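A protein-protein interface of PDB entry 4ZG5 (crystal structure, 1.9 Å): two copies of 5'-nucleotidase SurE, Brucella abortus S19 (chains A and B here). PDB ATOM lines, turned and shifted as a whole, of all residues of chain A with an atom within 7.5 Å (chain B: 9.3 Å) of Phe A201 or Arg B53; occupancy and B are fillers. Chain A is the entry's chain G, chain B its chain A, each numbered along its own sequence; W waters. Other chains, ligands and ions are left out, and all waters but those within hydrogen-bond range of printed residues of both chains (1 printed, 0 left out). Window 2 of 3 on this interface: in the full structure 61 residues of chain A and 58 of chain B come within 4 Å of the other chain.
Water W1 bridges N of Leu B54 (2.8 Å) and O of Pro A202 (3.0 Å).
OD2 of Asp A197 lies within salt-bridge range of NH2 of Arg B53 (2.7 Å).
The backbone NH of Leu B52 sits at hydrogen-bond distance from the backbone carbonyl oxygen of Phe A204, at 2.8 Å.
The guanidinium group (NH1) of Arg B53 lies within hydrogen-bond range of the backbone carbonyl oxygen (O) of Pro A202.
NH1 of Arg B53 sits at hydrogen-bond distance from O of Phe A201, at 3.5 Å.
Of chain B, only Arg B53 (2.7 Å) comes within 4 Å of Asp A197.
No residue of chain B comes within 4 Å of Arg A199.
No residue of chain B comes within 4 Å of Gly A200.
Phe A201 touches just one residue of chain B: Arg B53.
Printed residues of chain B within 4 Å of Tyr A203: Pro B51 (3.6 Å) and Leu B52 (3.4 Å).
Printed residues of chain B within 4 Å of Phe A204: Pro B51, Leu B52 and Met B74.
Of the printed residues of chain A, Pro B51 touches Tyr A203 (3.6 Å) and Phe A204 (3.4 Å).
Of the printed residues of chain A, Leu B52 touches Tyr A203 (3.4 Å) and Phe A204 (2.8 Å).
Arg B53 touches just these residues of chain A: Asp A197 (2.7 Å), Phe A201 (3.5 Å) and Pro A202 (3.1 Å).
The nearest residue of chain B that does not touch Phe A201 is Leu B52 (7.7 Å).
The nearest residue of chain A that does not touch Arg B53 is Tyr A203 (4.03 Å).
The nearest printed residue of chain A that does not touch Pro B51 is Pro A202 (6.8 Å).
The side-chain carboxylate (OD1) of Asp A197 lies within hydrogen-bond range of the backbone NH (N) of Arg A199, at 2.9 Å.
N of Gly A200 is in hydrogen-bond range of OD1 of Asp A197 (3.1 Å).
The backbone carbonyl oxygen of Arg B53 sits at hydrogen-bond distance from the backbone NH of Arg B65 (3.0 Å).
OD1 of Asp A197 sits at hydrogen-bond distance from N of Phe A201 (2.9 Å).
The backbone NH of Arg A195 lies within hydrogen-bond range of the backbone carbonyl oxygen of Tyr A203, 2.8 Å away.
No position is printed for both chains.
Of the 8 pairs that touch across the chains among the printed residues, none has its exchanged pair printed and touching as well.
Pro B51 touches Tyr A203.
Leu B52 touches Tyr A203.
CA of Pro B51 touches O of Phe A204, at 3.4 Å.
Met B74 touches Phe A204 (CE to CD2, 3.7 Å).
Printed residues of chain B that touch a printed residue of chain A: Pro B51, Leu B52, Arg B53 and Met B74.
Hydrophobic or aromatic side chains of chain B within 4 Å of the printed part of chain A: Pro B51, Leu B52 and Met B74.
Of the 10 printed residues of chain A, 5 touch a printed residue of chain B.
Hydrophobic or aromatic side chains of chain A that line the printed part of chain B: Phe A201, Tyr A203 and Phe A204.
Among the printed residues, 8 pairs touch across the chains.
Among the printed residues, Asp or Glu carboxylates within 4 Å of a Lys or Arg side-chain nitrogen of the other chain: Asp A197 with Arg B53.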
ATOM      1  N   ARG A 195      -8.609 -24.847 -21.894  1.00  0.00           N
ATOM      2  CA  ARG A 195      -8.963 -25.329 -20.565  1.00  0.00           C
ATOM      3  C   ARG A 195      -7.780 -26.032 -19.850  1.00  0.00           C
ATOM      4  O   ARG A 195      -6.739 -26.243 -20.450  1.00  0.00           O
ATOM      5  CB  ARG A 195     -10.085 -26.405 -20.705  1.00  0.00           C
ATOM      6  CG  ARG A 195     -11.174 -26.161 -21.783  1.00  0.00           C
ATOM      7  CD  ARG A 195     -12.376 -25.515 -21.135  1.00  0.00           C
ATOM      8  NE  ARG A 195     -13.437 -25.216 -22.074  1.00  0.00           N
ATOM      9  CZ  ARG A 195     -14.511 -25.977 -22.333  1.00  0.00           C
ATOM     10  NH1 ARG A 195     -14.803 -27.116 -21.669  1.00  0.00           N
ATOM     11  NH2 ARG A 195     -15.376 -25.532 -23.254  1.00  0.00           N
ATOM     12  N   ARG A 196      -8.059 -26.532 -18.654  1.00  0.00           N
ATOM     13  CA  ARG A 196      -7.172 -27.415 -17.875  1.00  0.00           C
ATOM     14  C   ARG A 196      -7.904 -28.697 -17.433  1.00  0.00           C
ATOM     15  O   ARG A 196      -9.064 -28.657 -16.995  1.00  0.00           O
ATOM     16  CB  ARG A 196      -6.729 -26.711 -16.630  1.00  0.00           C
ATOM     17  CG  ARG A 196      -6.117 -25.374 -16.880  1.00  0.00           C
ATOM     18  CD  ARG A 196      -4.818 -25.550 -17.631  1.00  0.00           C
ATOM     19  NE  ARG A 196      -3.971 -24.478 -17.232  1.00  0.00           N
ATOM     20  CZ  ARG A 196      -3.377 -24.441 -15.983  1.00  0.00           C
ATOM     21  NH1 ARG A 196      -3.476 -25.480 -15.089  1.00  0.00           N
ATOM     22  NH2 ARG A 196      -2.650 -23.378 -15.598  1.00  0.00           N
ATOM     23  N   ASP A 197      -7.238 -29.825 -17.576  1.00  0.00           N
ATOM     24  CA  ASP A 197      -7.869 -31.128 -17.324  1.00  0.00           C
ATOM     25  C   ASP A 197      -7.892 -31.398 -15.816  1.00  0.00           C
ATOM     26  O   ASP A 197      -7.505 -30.533 -15.043  1.00  0.00           O
ATOM     27  CB  ASP A 197      -7.252 -32.222 -18.165  1.00  0.00           C
ATOM     28  CG  ASP A 197      -5.844 -32.565 -17.806  1.00  0.00           C
ATOM     29  OD1 ASP A 197      -5.406 -32.238 -16.696  1.00  0.00           O
ATOM     30  OD2 ASP A 197      -5.201 -33.180 -18.709  1.00  0.00           O
ATOM     31  N   GLY A 198      -8.380 -32.566 -15.408  1.00  0.00           N
ATOM     32  CA  GLY A 198      -8.446 -32.931 -13.987  1.00  0.00           C
ATOM     33  C   GLY A 198      -7.106 -32.982 -13.282  1.00  0.00           C
ATOM     34  O   GLY A 198      -7.053 -32.778 -12.067  1.00  0.00           O
ATOM     35  N   ARG A 199      -6.000 -33.159 -14.024  1.00  0.00           N
ATOM     36  CA  ARG A 199      -4.644 -33.023 -13.458  1.00  0.00           C
ATOM     37  C   ARG A 199      -3.986 -31.674 -13.641  1.00  0.00           C
ATOM     38  O   ARG A 199      -2.781 -31.544 -13.424  1.00  0.00           O
ATOM     39  CB  ARG A 199      -3.787 -34.149 -14.020  1.00  0.00           C
ATOM     40  CG  ARG A 199      -4.436 -35.482 -13.701  1.00  0.00           C
ATOM     41  CD  ARG A 199      -3.596 -36.682 -14.083  1.00  0.00           C
ATOM     42  NE  ARG A 199      -3.348 -36.703 -15.520  1.00  0.00           N
ATOM     43  CZ  ARG A 199      -2.341 -37.359 -16.096  1.00  0.00           C
ATOM     44  NH1 ARG A 199      -1.447 -38.045 -15.373  1.00  0.00           N
ATOM     45  NH2 ARG A 199      -2.233 -37.336 -17.403  1.00  0.00           N
ATOM     46  N   GLY A 200      -4.728 -30.673 -14.117  1.00  0.00           N
ATOM     47  CA  GLY A 200      -4.149 -29.316 -14.268  1.00  0.00           C
ATOM     48  C   GLY A 200      -3.503 -29.052 -15.630  1.00  0.00           C
ATOM     49  O   GLY A 200      -2.980 -27.992 -15.850  1.00  0.00           O
ATOM     50  N   PHE A 201      -3.510 -30.037 -16.555  1.00  0.00           N
ATOM     51  CA  PHE A 201      -2.788 -29.880 -17.791  1.00  0.00           C
ATOM     52  C   PHE A 201      -3.656 -29.231 -18.871  1.00  0.00           C
ATOM     53  O   PHE A 201      -4.808 -29.623 -19.040  1.00  0.00           O
ATOM     54  CB  PHE A 201      -2.306 -31.211 -18.363  1.00  0.00           C
ATOM     55  CG  PHE A 201      -1.330 -31.925 -17.453  1.00  0.00           C
ATOM     56  CD1 PHE A 201      -0.124 -31.359 -17.134  1.00  0.00           C
ATOM     57  CD2 PHE A 201      -1.638 -33.175 -16.938  1.00  0.00           C
ATOM     58  CE1 PHE A 201       0.783 -31.994 -16.278  1.00  0.00           C
ATOM     59  CE2 PHE A 201      -0.748 -33.826 -16.096  1.00  0.00           C
ATOM     60  CZ  PHE A 201       0.460 -33.225 -15.751  1.00  0.00           C
ATOM     61  N   PRO A 202      -3.022 -28.399 -19.680  1.00  0.00           N
ATOM     62  CA  PRO A 202      -3.800 -27.642 -20.667  1.00  0.00           C
ATOM     63  C   PRO A 202      -4.283 -28.476 -21.814  1.00  0.00           C
ATOM     64  O   PRO A 202      -3.599 -29.429 -22.281  1.00  0.00           O
ATOM     65  CB  PRO A 202      -2.825 -26.549 -21.185  1.00  0.00           C
ATOM     66  CG  PRO A 202      -1.498 -26.797 -20.543  1.00  0.00           C
ATOM     67  CD  PRO A 202      -1.655 -27.843 -19.456  1.00  0.00           C
ATOM     68  N   TYR A 203      -5.433 -28.100 -22.299  1.00  0.00           N
ATOM     69  CA  TYR A 203      -5.943 -28.551 -23.561  1.00  0.00           C
ATOM     70  C   TYR A 203      -6.862 -27.537 -24.245  1.00  0.00           C
ATOM     71  O   TYR A 203      -7.223 -26.523 -23.626  1.00  0.00           O
ATOM     72  CB  TYR A 203      -6.690 -29.852 -23.346  1.00  0.00           C
ATOM     73  CG  TYR A 203      -7.956 -29.784 -22.587  1.00  0.00           C
ATOM     74  CD1 TYR A 203      -9.199 -29.850 -23.249  1.00  0.00           C
ATOM     75  CD2 TYR A 203      -7.970 -29.810 -21.192  1.00  0.00           C
ATOM     76  CE1 TYR A 203     -10.365 -29.804 -22.523  1.00  0.00           C
ATOM     77  CE2 TYR A 203      -9.169 -29.775 -20.466  1.00  0.00           C
ATOM     78  CZ  TYR A 203     -10.352 -29.810 -21.170  1.00  0.00           C
ATOM     79  OH  TYR A 203     -11.563 -29.793 -20.474  1.00  0.00           O
ATOM     80  N   PHE A 204      -7.211 -27.840 -25.502  1.00  0.00           N
ATOM     81  CA  PHE A 204      -8.084 -27.002 -26.289  1.00  0.00           C
ATOM     82  C   PHE A 204      -9.211 -27.808 -26.966  1.00  0.00           C
ATOM     83  O   PHE A 204      -9.031 -28.987 -27.357  1.00  0.00           O
ATOM     84  CB  PHE A 204      -7.324 -26.266 -27.373  1.00  0.00           C
ATOM     85  CG  PHE A 204      -6.227 -25.386 -26.874  1.00  0.00           C
ATOM     86  CD1 PHE A 204      -6.389 -24.019 -26.774  1.00  0.00           C
ATOM     87  CD2 PHE A 204      -4.983 -25.944 -26.537  1.00  0.00           C
ATOM     88  CE1 PHE A 204      -5.347 -23.199 -26.377  1.00  0.00           C
ATOM     89  CE2 PHE A 204      -3.935 -25.118 -26.182  1.00  0.00           C
ATOM     90  CZ  PHE A 204      -4.137 -23.776 -26.042  1.00  0.00           C
ATOM     91  N   VAL B  33       4.348 -24.919 -35.923  1.00  0.00           N
ATOM     92  CA  VAL B  33       3.338 -25.731 -35.212  1.00  0.00           C
ATOM     93  C   VAL B  33       3.088 -26.958 -36.113  1.00  0.00           C
ATOM     94  O   VAL B  33       2.537 -26.826 -37.212  1.00  0.00           O
ATOM     95  CB  VAL B  33       1.992 -24.999 -34.990  1.00  0.00           C
ATOM     96  CG1 VAL B  33       1.035 -25.864 -34.149  1.00  0.00           C
ATOM     97  CG2 VAL B  33       2.185 -23.654 -34.293  1.00  0.00           C
ATOM     98  N   ALA B  34       3.480 -28.125 -35.632  1.00  0.00           N
ATOM     99  CA  ALA B  34       3.471 -29.344 -36.424  1.00  0.00           C
ATOM    100  C   ALA B  34       2.942 -30.500 -35.674  1.00  0.00           C
ATOM    101  O   ALA B  34       3.043 -30.543 -34.438  1.00  0.00           O
ATOM    102  CB  ALA B  34       4.889 -29.663 -36.933  1.00  0.00           C
ATOM    103  N   PRO B  35       2.469 -31.502 -36.389  1.00  0.00           N
ATOM    104  CA  PRO B  35       1.952 -32.666 -35.671  1.00  0.00           C
ATOM    105  C   PRO B  35       2.950 -33.420 -34.856  1.00  0.00           C
ATOM    106  O   PRO B  35       4.192 -33.398 -35.146  1.00  0.00           O
ATOM    107  CB  PRO B  35       1.403 -33.577 -36.784  1.00  0.00           C
ATOM    108  CG  PRO B  35       1.111 -32.692 -37.899  1.00  0.00           C
ATOM    109  CD  PRO B  35       2.220 -31.627 -37.807  1.00  0.00           C
ATOM    110  N   GLU B  36       2.454 -34.090 -33.811  1.00  0.00           N
ATOM    111  CA  GLU B  36       3.335 -34.959 -33.038  1.00  0.00           C
ATOM    112  C   GLU B  36       3.849 -36.100 -33.891  1.00  0.00           C
ATOM    113  O   GLU B  36       4.984 -36.483 -33.745  1.00  0.00           O
ATOM    114  CB  GLU B  36       2.641 -35.469 -31.745  1.00  0.00           C
ATOM    115  CG  GLU B  36       2.458 -34.402 -30.643  1.00  0.00           C
ATOM    116  CD  GLU B  36       3.688 -34.096 -29.842  1.00  0.00           C
ATOM    117  OE1 GLU B  36       4.788 -34.553 -30.166  1.00  0.00           O
ATOM    118  OE2 GLU B  36       3.530 -33.425 -28.787  1.00  0.00           O
ATOM    119  N   THR B  47      -9.717 -32.006 -35.761  1.00  0.00           N
ATOM    120  CA  THR B  47     -10.005 -32.768 -34.543  1.00  0.00           C
ATOM    121  C   THR B  47     -11.123 -31.954 -33.805  1.00  0.00           C
ATOM    122  O   THR B  47     -10.869 -30.900 -33.189  1.00  0.00           O
ATOM    123  CB  THR B  47      -8.737 -32.877 -33.696  1.00  0.00           C
ATOM    124  OG1 THR B  47      -7.708 -33.443 -34.483  1.00  0.00           O
ATOM    125  CG2 THR B  47      -8.972 -33.683 -32.447  1.00  0.00           C
ATOM    126  N   GLU B  50     -12.182 -34.841 -29.762  1.00  0.00           N
ATOM    127  CA  GLU B  50     -11.220 -35.012 -28.736  1.00  0.00           C
ATOM    128  C   GLU B  50     -10.457 -33.687 -28.537  1.00  0.00           C
ATOM    129  O   GLU B  50     -10.332 -32.916 -29.456  1.00  0.00           O
ATOM    130  CB  GLU B  50     -10.168 -36.030 -29.167  1.00  0.00           C
ATOM    131  CG  GLU B  50     -10.788 -37.364 -29.478  1.00  0.00           C
ATOM    132  CD  GLU B  50      -9.752 -38.318 -29.986  1.00  0.00           C
ATOM    133  OE1 GLU B  50      -8.548 -38.157 -29.606  1.00  0.00           O
ATOM    134  OE2 GLU B  50     -10.143 -39.216 -30.777  1.00  0.00           O
ATOM    135  N   PRO B  51      -9.923 -33.487 -27.376  1.00  0.00           N
ATOM    136  CA  PRO B  51      -9.062 -32.347 -27.124  1.00  0.00           C
ATOM    137  C   PRO B  51      -7.829 -32.283 -27.888  1.00  0.00           C
ATOM    138  O   PRO B  51      -7.195 -33.309 -28.199  1.00  0.00           O
ATOM    139  CB  PRO B  51      -8.672 -32.499 -25.646  1.00  0.00           C
ATOM    140  CG  PRO B  51      -9.637 -33.454 -25.081  1.00  0.00           C
ATOM    141  CD  PRO B  51     -10.036 -34.361 -26.195  1.00  0.00           C
ATOM    142  N   LEU B  52      -7.459 -31.097 -28.213  1.00  0.00           N
ATOM    143  CA  LEU B  52      -6.128 -30.876 -28.756  1.00  0.00           C
ATOM    144  C   LEU B  52      -5.104 -30.631 -27.640  1.00  0.00           C
ATOM    145  O   LEU B  52      -5.364 -29.844 -26.705  1.00  0.00           O
ATOM    146  CB  LEU B  52      -6.198 -29.637 -29.683  1.00  0.00           C
ATOM    147  CG  LEU B  52      -6.881 -29.899 -31.023  1.00  0.00           C
ATOM    148  CD1 LEU B  52      -7.165 -28.580 -31.725  1.00  0.00           C
ATOM    149  CD2 LEU B  52      -6.072 -30.831 -31.906  1.00  0.00           C
ATOM    150  N   ARG B  53      -3.918 -31.251 -27.737  1.00  0.00           N
ATOM    151  CA  ARG B  53      -2.834 -31.053 -26.764  1.00  0.00           C
ATOM    152  C   ARG B  53      -1.649 -30.430 -27.444  1.00  0.00           C
ATOM    153  O   ARG B  53      -1.072 -30.988 -28.395  1.00  0.00           O
ATOM    154  CB  ARG B  53      -2.407 -32.404 -26.124  1.00  0.00           C
ATOM    155  CG  ARG B  53      -3.520 -33.139 -25.384  1.00  0.00           C
ATOM    156  CD  ARG B  53      -3.758 -32.524 -24.059  1.00  0.00           C
ATOM    157  NE  ARG B  53      -4.619 -33.342 -23.234  1.00  0.00           N
ATOM    158  CZ  ARG B  53      -4.760 -33.207 -21.915  1.00  0.00           C
ATOM    159  NH1 ARG B  53      -4.171 -32.238 -21.233  1.00  0.00           N
ATOM    160  NH2 ARG B  53      -5.601 -34.026 -21.285  1.00  0.00           N
ATOM    161  N   LEU B  54      -1.227 -29.318 -26.922  1.00  0.00           N
ATOM    162  CA  LEU B  54      -0.184 -28.483 -27.495  1.00  0.00           C
ATOM    163  C   LEU B  54       1.039 -28.619 -26.635  1.00  0.00           C
ATOM    164  O   LEU B  54       0.925 -28.506 -25.443  1.00  0.00           O
ATOM    165  CB  LEU B  54      -0.628 -27.046 -27.470  1.00  0.00           C
ATOM    166  CG  LEU B  54       0.365 -25.999 -28.041  1.00  0.00           C
ATOM    167  CD1 LEU B  54       0.537 -26.178 -29.523  1.00  0.00           C
ATOM    168  CD2 LEU B  54      -0.035 -24.569 -27.656  1.00  0.00           C
ATOM    169  N   ARG B  55       2.203 -28.868 -27.238  1.00  0.00           N
ATOM    170  CA  ARG B  55       3.437 -29.058 -26.472  1.00  0.00           C
ATOM    171  C   ARG B  55       4.469 -28.061 -26.946  1.00  0.00           C
ATOM    172  O   ARG B  55       4.782 -28.020 -28.121  1.00  0.00           O
ATOM    173  CB  ARG B  55       3.994 -30.451 -26.651  1.00  0.00           C
ATOM    174  CG  ARG B  55       5.326 -30.678 -25.970  1.00  0.00           C
ATOM    175  CD  ARG B  55       5.691 -32.161 -26.006  1.00  0.00           C
ATOM    176  NE  ARG B  55       5.904 -32.657 -27.379  1.00  0.00           N
ATOM    177  CZ  ARG B  55       7.094 -32.722 -27.983  1.00  0.00           C
ATOM    178  NH1 ARG B  55       8.184 -32.260 -27.412  1.00  0.00           N
ATOM    179  NH2 ARG B  55       7.179 -33.229 -29.176  1.00  0.00           N
ATOM    180  N   GLN B  56       4.974 -27.239 -26.045  1.00  0.00           N
ATOM    181  CA  GLN B  56       5.905 -26.219 -26.431  1.00  0.00           C
ATOM    182  C   GLN B  56       7.324 -26.732 -26.345  1.00  0.00           C
ATOM    183  O   GLN B  56       7.702 -27.271 -25.338  1.00  0.00           O
ATOM    184  CB  GLN B  56       5.754 -25.039 -25.487  1.00  0.00           C
ATOM    185  CG  GLN B  56       6.703 -23.918 -25.793  1.00  0.00           C
ATOM    186  CD  GLN B  56       6.335 -22.636 -25.034  1.00  0.00           C
ATOM    187  OE1 GLN B  56       5.165 -22.370 -24.811  1.00  0.00           O
ATOM    188  NE2 GLN B  56       7.325 -21.822 -24.662  1.00  0.00           N
ATOM    189  N   PHE B  62       6.387 -25.681 -31.621  1.00  0.00           N
ATOM    190  CA  PHE B  62       5.331 -26.316 -30.903  1.00  0.00           C
ATOM    191  C   PHE B  62       4.930 -27.561 -31.650  1.00  0.00           C
ATOM    192  O   PHE B  62       4.870 -27.555 -32.891  1.00  0.00           O
ATOM    193  CB  PHE B  62       4.085 -25.378 -30.880  1.00  0.00           C
ATOM    194  CG  PHE B  62       4.280 -24.136 -30.137  1.00  0.00           C
ATOM    195  CD1 PHE B  62       3.880 -24.021 -28.781  1.00  0.00           C
ATOM    196  CD2 PHE B  62       4.980 -23.078 -30.714  1.00  0.00           C
ATOM    197  CE1 PHE B  62       4.127 -22.842 -28.093  1.00  0.00           C
ATOM    198  CE2 PHE B  62       5.185 -21.881 -30.024  1.00  0.00           C
ATOM    199  CZ  PHE B  62       4.791 -21.779 -28.690  1.00  0.00           C
ATOM    200  N   ALA B  63       4.622 -28.626 -30.903  1.00  0.00           N
ATOM    201  CA  ALA B  63       4.056 -29.809 -31.463  1.00  0.00           C
ATOM    202  C   ALA B  63       2.598 -29.895 -31.024  1.00  0.00           C
ATOM    203  O   ALA B  63       2.265 -29.500 -29.901  1.00  0.00           O
ATOM    204  CB  ALA B  63       4.846 -31.036 -31.006  1.00  0.00           C
ATOM    205  N   LEU B  64       1.722 -30.420 -31.885  1.00  0.00           N
ATOM    206  CA  LEU B  64       0.309 -30.517 -31.554  1.00  0.00           C
ATOM    207  C   LEU B  64      -0.172 -31.900 -31.901  1.00  0.00           C
ATOM    208  O   LEU B  64       0.115 -32.450 -32.968  1.00  0.00           O
ATOM    209  CB  LEU B  64      -0.482 -29.499 -32.390  1.00  0.00           C
ATOM    210  CG  LEU B  64      -1.987 -29.490 -32.126  1.00  0.00           C
ATOM    211  CD1 LEU B  64      -2.267 -28.932 -30.723  1.00  0.00           C
ATOM    212  CD2 LEU B  64      -2.618 -28.589 -33.198  1.00  0.00           C
ATOM    213  N   ARG B  65      -0.898 -32.475 -30.993  1.00  0.00           N
ATOM    214  CA  ARG B  65      -1.412 -33.807 -31.159  1.00  0.00           C
ATOM    215  C   ARG B  65      -2.704 -33.667 -31.996  1.00  0.00           C
ATOM    216  O   ARG B  65      -3.761 -33.562 -31.460  1.00  0.00           O
ATOM    217  CB  ARG B  65      -1.697 -34.510 -29.845  1.00  0.00           C
ATOM    218  CG  ARG B  65      -2.454 -35.902 -30.059  1.00  0.00           C
ATOM    219  CD  ARG B  65      -1.520 -37.027 -30.409  1.00  0.00           C
ATOM    220  NE  ARG B  65      -0.433 -37.135 -29.436  1.00  0.00           N
ATOM    221  CZ  ARG B  65       0.636 -37.926 -29.595  1.00  0.00           C
ATOM    222  NH1 ARG B  65       0.729 -38.720 -30.639  1.00  0.00           N
ATOM    223  NH2 ARG B  65       1.613 -37.897 -28.721  1.00  0.00           N
ATOM    224  N   GLY B  66      -2.532 -33.571 -33.314  1.00  0.00           N
ATOM    225  CA  GLY B  66      -3.601 -33.158 -34.188  1.00  0.00           C
ATOM    226  C   GLY B  66      -3.079 -33.171 -35.595  1.00  0.00           C
ATOM    227  O   GLY B  66      -1.920 -33.556 -35.851  1.00  0.00           O
ATOM    228  N   THR B  67      -3.931 -32.752 -36.495  1.00  0.00           N
ATOM    229  CA  THR B  67      -3.645 -32.718 -37.945  1.00  0.00           C
ATOM    230  C   THR B  67      -2.906 -31.473 -38.396  1.00  0.00           C
ATOM    231  O   THR B  67      -2.854 -30.472 -37.664  1.00  0.00           O
ATOM    232  CB  THR B  67      -4.956 -32.823 -38.735  1.00  0.00           C
ATOM    233  OG1 THR B  67      -5.734 -31.598 -38.624  1.00  0.00           O
ATOM    234  CG2 THR B  67      -5.816 -34.092 -38.225  1.00  0.00           C
ATOM    235  N   ASP B  70      -5.399 -28.716 -38.005  1.00  0.00           N
ATOM    236  CA  ASP B  70      -5.456 -28.293 -36.615  1.00  0.00           C
ATOM    237  C   ASP B  70      -4.235 -27.335 -36.323  1.00  0.00           C
ATOM    238  O   ASP B  70      -4.379 -26.368 -35.591  1.00  0.00           O
ATOM    239  CB  ASP B  70      -5.358 -29.438 -35.623  1.00  0.00           C
ATOM    240  CG  ASP B  70      -6.544 -30.424 -35.666  1.00  0.00           C
ATOM    241  OD1 ASP B  70      -7.685 -30.006 -35.783  1.00  0.00           O
ATOM    242  OD2 ASP B  70      -6.249 -31.606 -35.499  1.00  0.00           O
ATOM    243  N   CYS B  71      -3.076 -27.700 -36.825  1.00  0.00           N
ATOM    244  CA  CYS B  71      -1.845 -26.947 -36.582  1.00  0.00           C
ATOM    245  C   CYS B  71      -1.919 -25.539 -37.084  1.00  0.00           C
ATOM    246  O   CYS B  71      -1.532 -24.599 -36.364  1.00  0.00           O
ATOM    247  CB  CYS B  71      -0.629 -27.665 -37.189  1.00  0.00           C
ATOM    248  SG  CYS B  71      -0.134 -29.191 -36.338  1.00  0.00           S
ATOM    249  N   MET B  74      -4.418 -23.553 -34.892  1.00  0.00           N
ATOM    250  CA  MET B  74      -3.771 -23.288 -33.633  1.00  0.00           C
ATOM    251  C   MET B  74      -2.719 -22.201 -33.742  1.00  0.00           C
ATOM    252  O   MET B  74      -2.648 -21.281 -32.903  1.00  0.00           O
ATOM    253  CB  MET B  74      -3.105 -24.556 -33.145  1.00  0.00           C
ATOM    254  CG  MET B  74      -2.283 -24.516 -31.897  1.00  0.00           C
ATOM    255  SD  MET B  74      -3.182 -23.973 -30.371  1.00  0.00           S
ATOM    256  CE  MET B  74      -4.279 -25.378 -30.141  1.00  0.00           C
HETATM  257  O   HOH W   1      -2.556 -28.149 -24.732  1.00  0.00           O
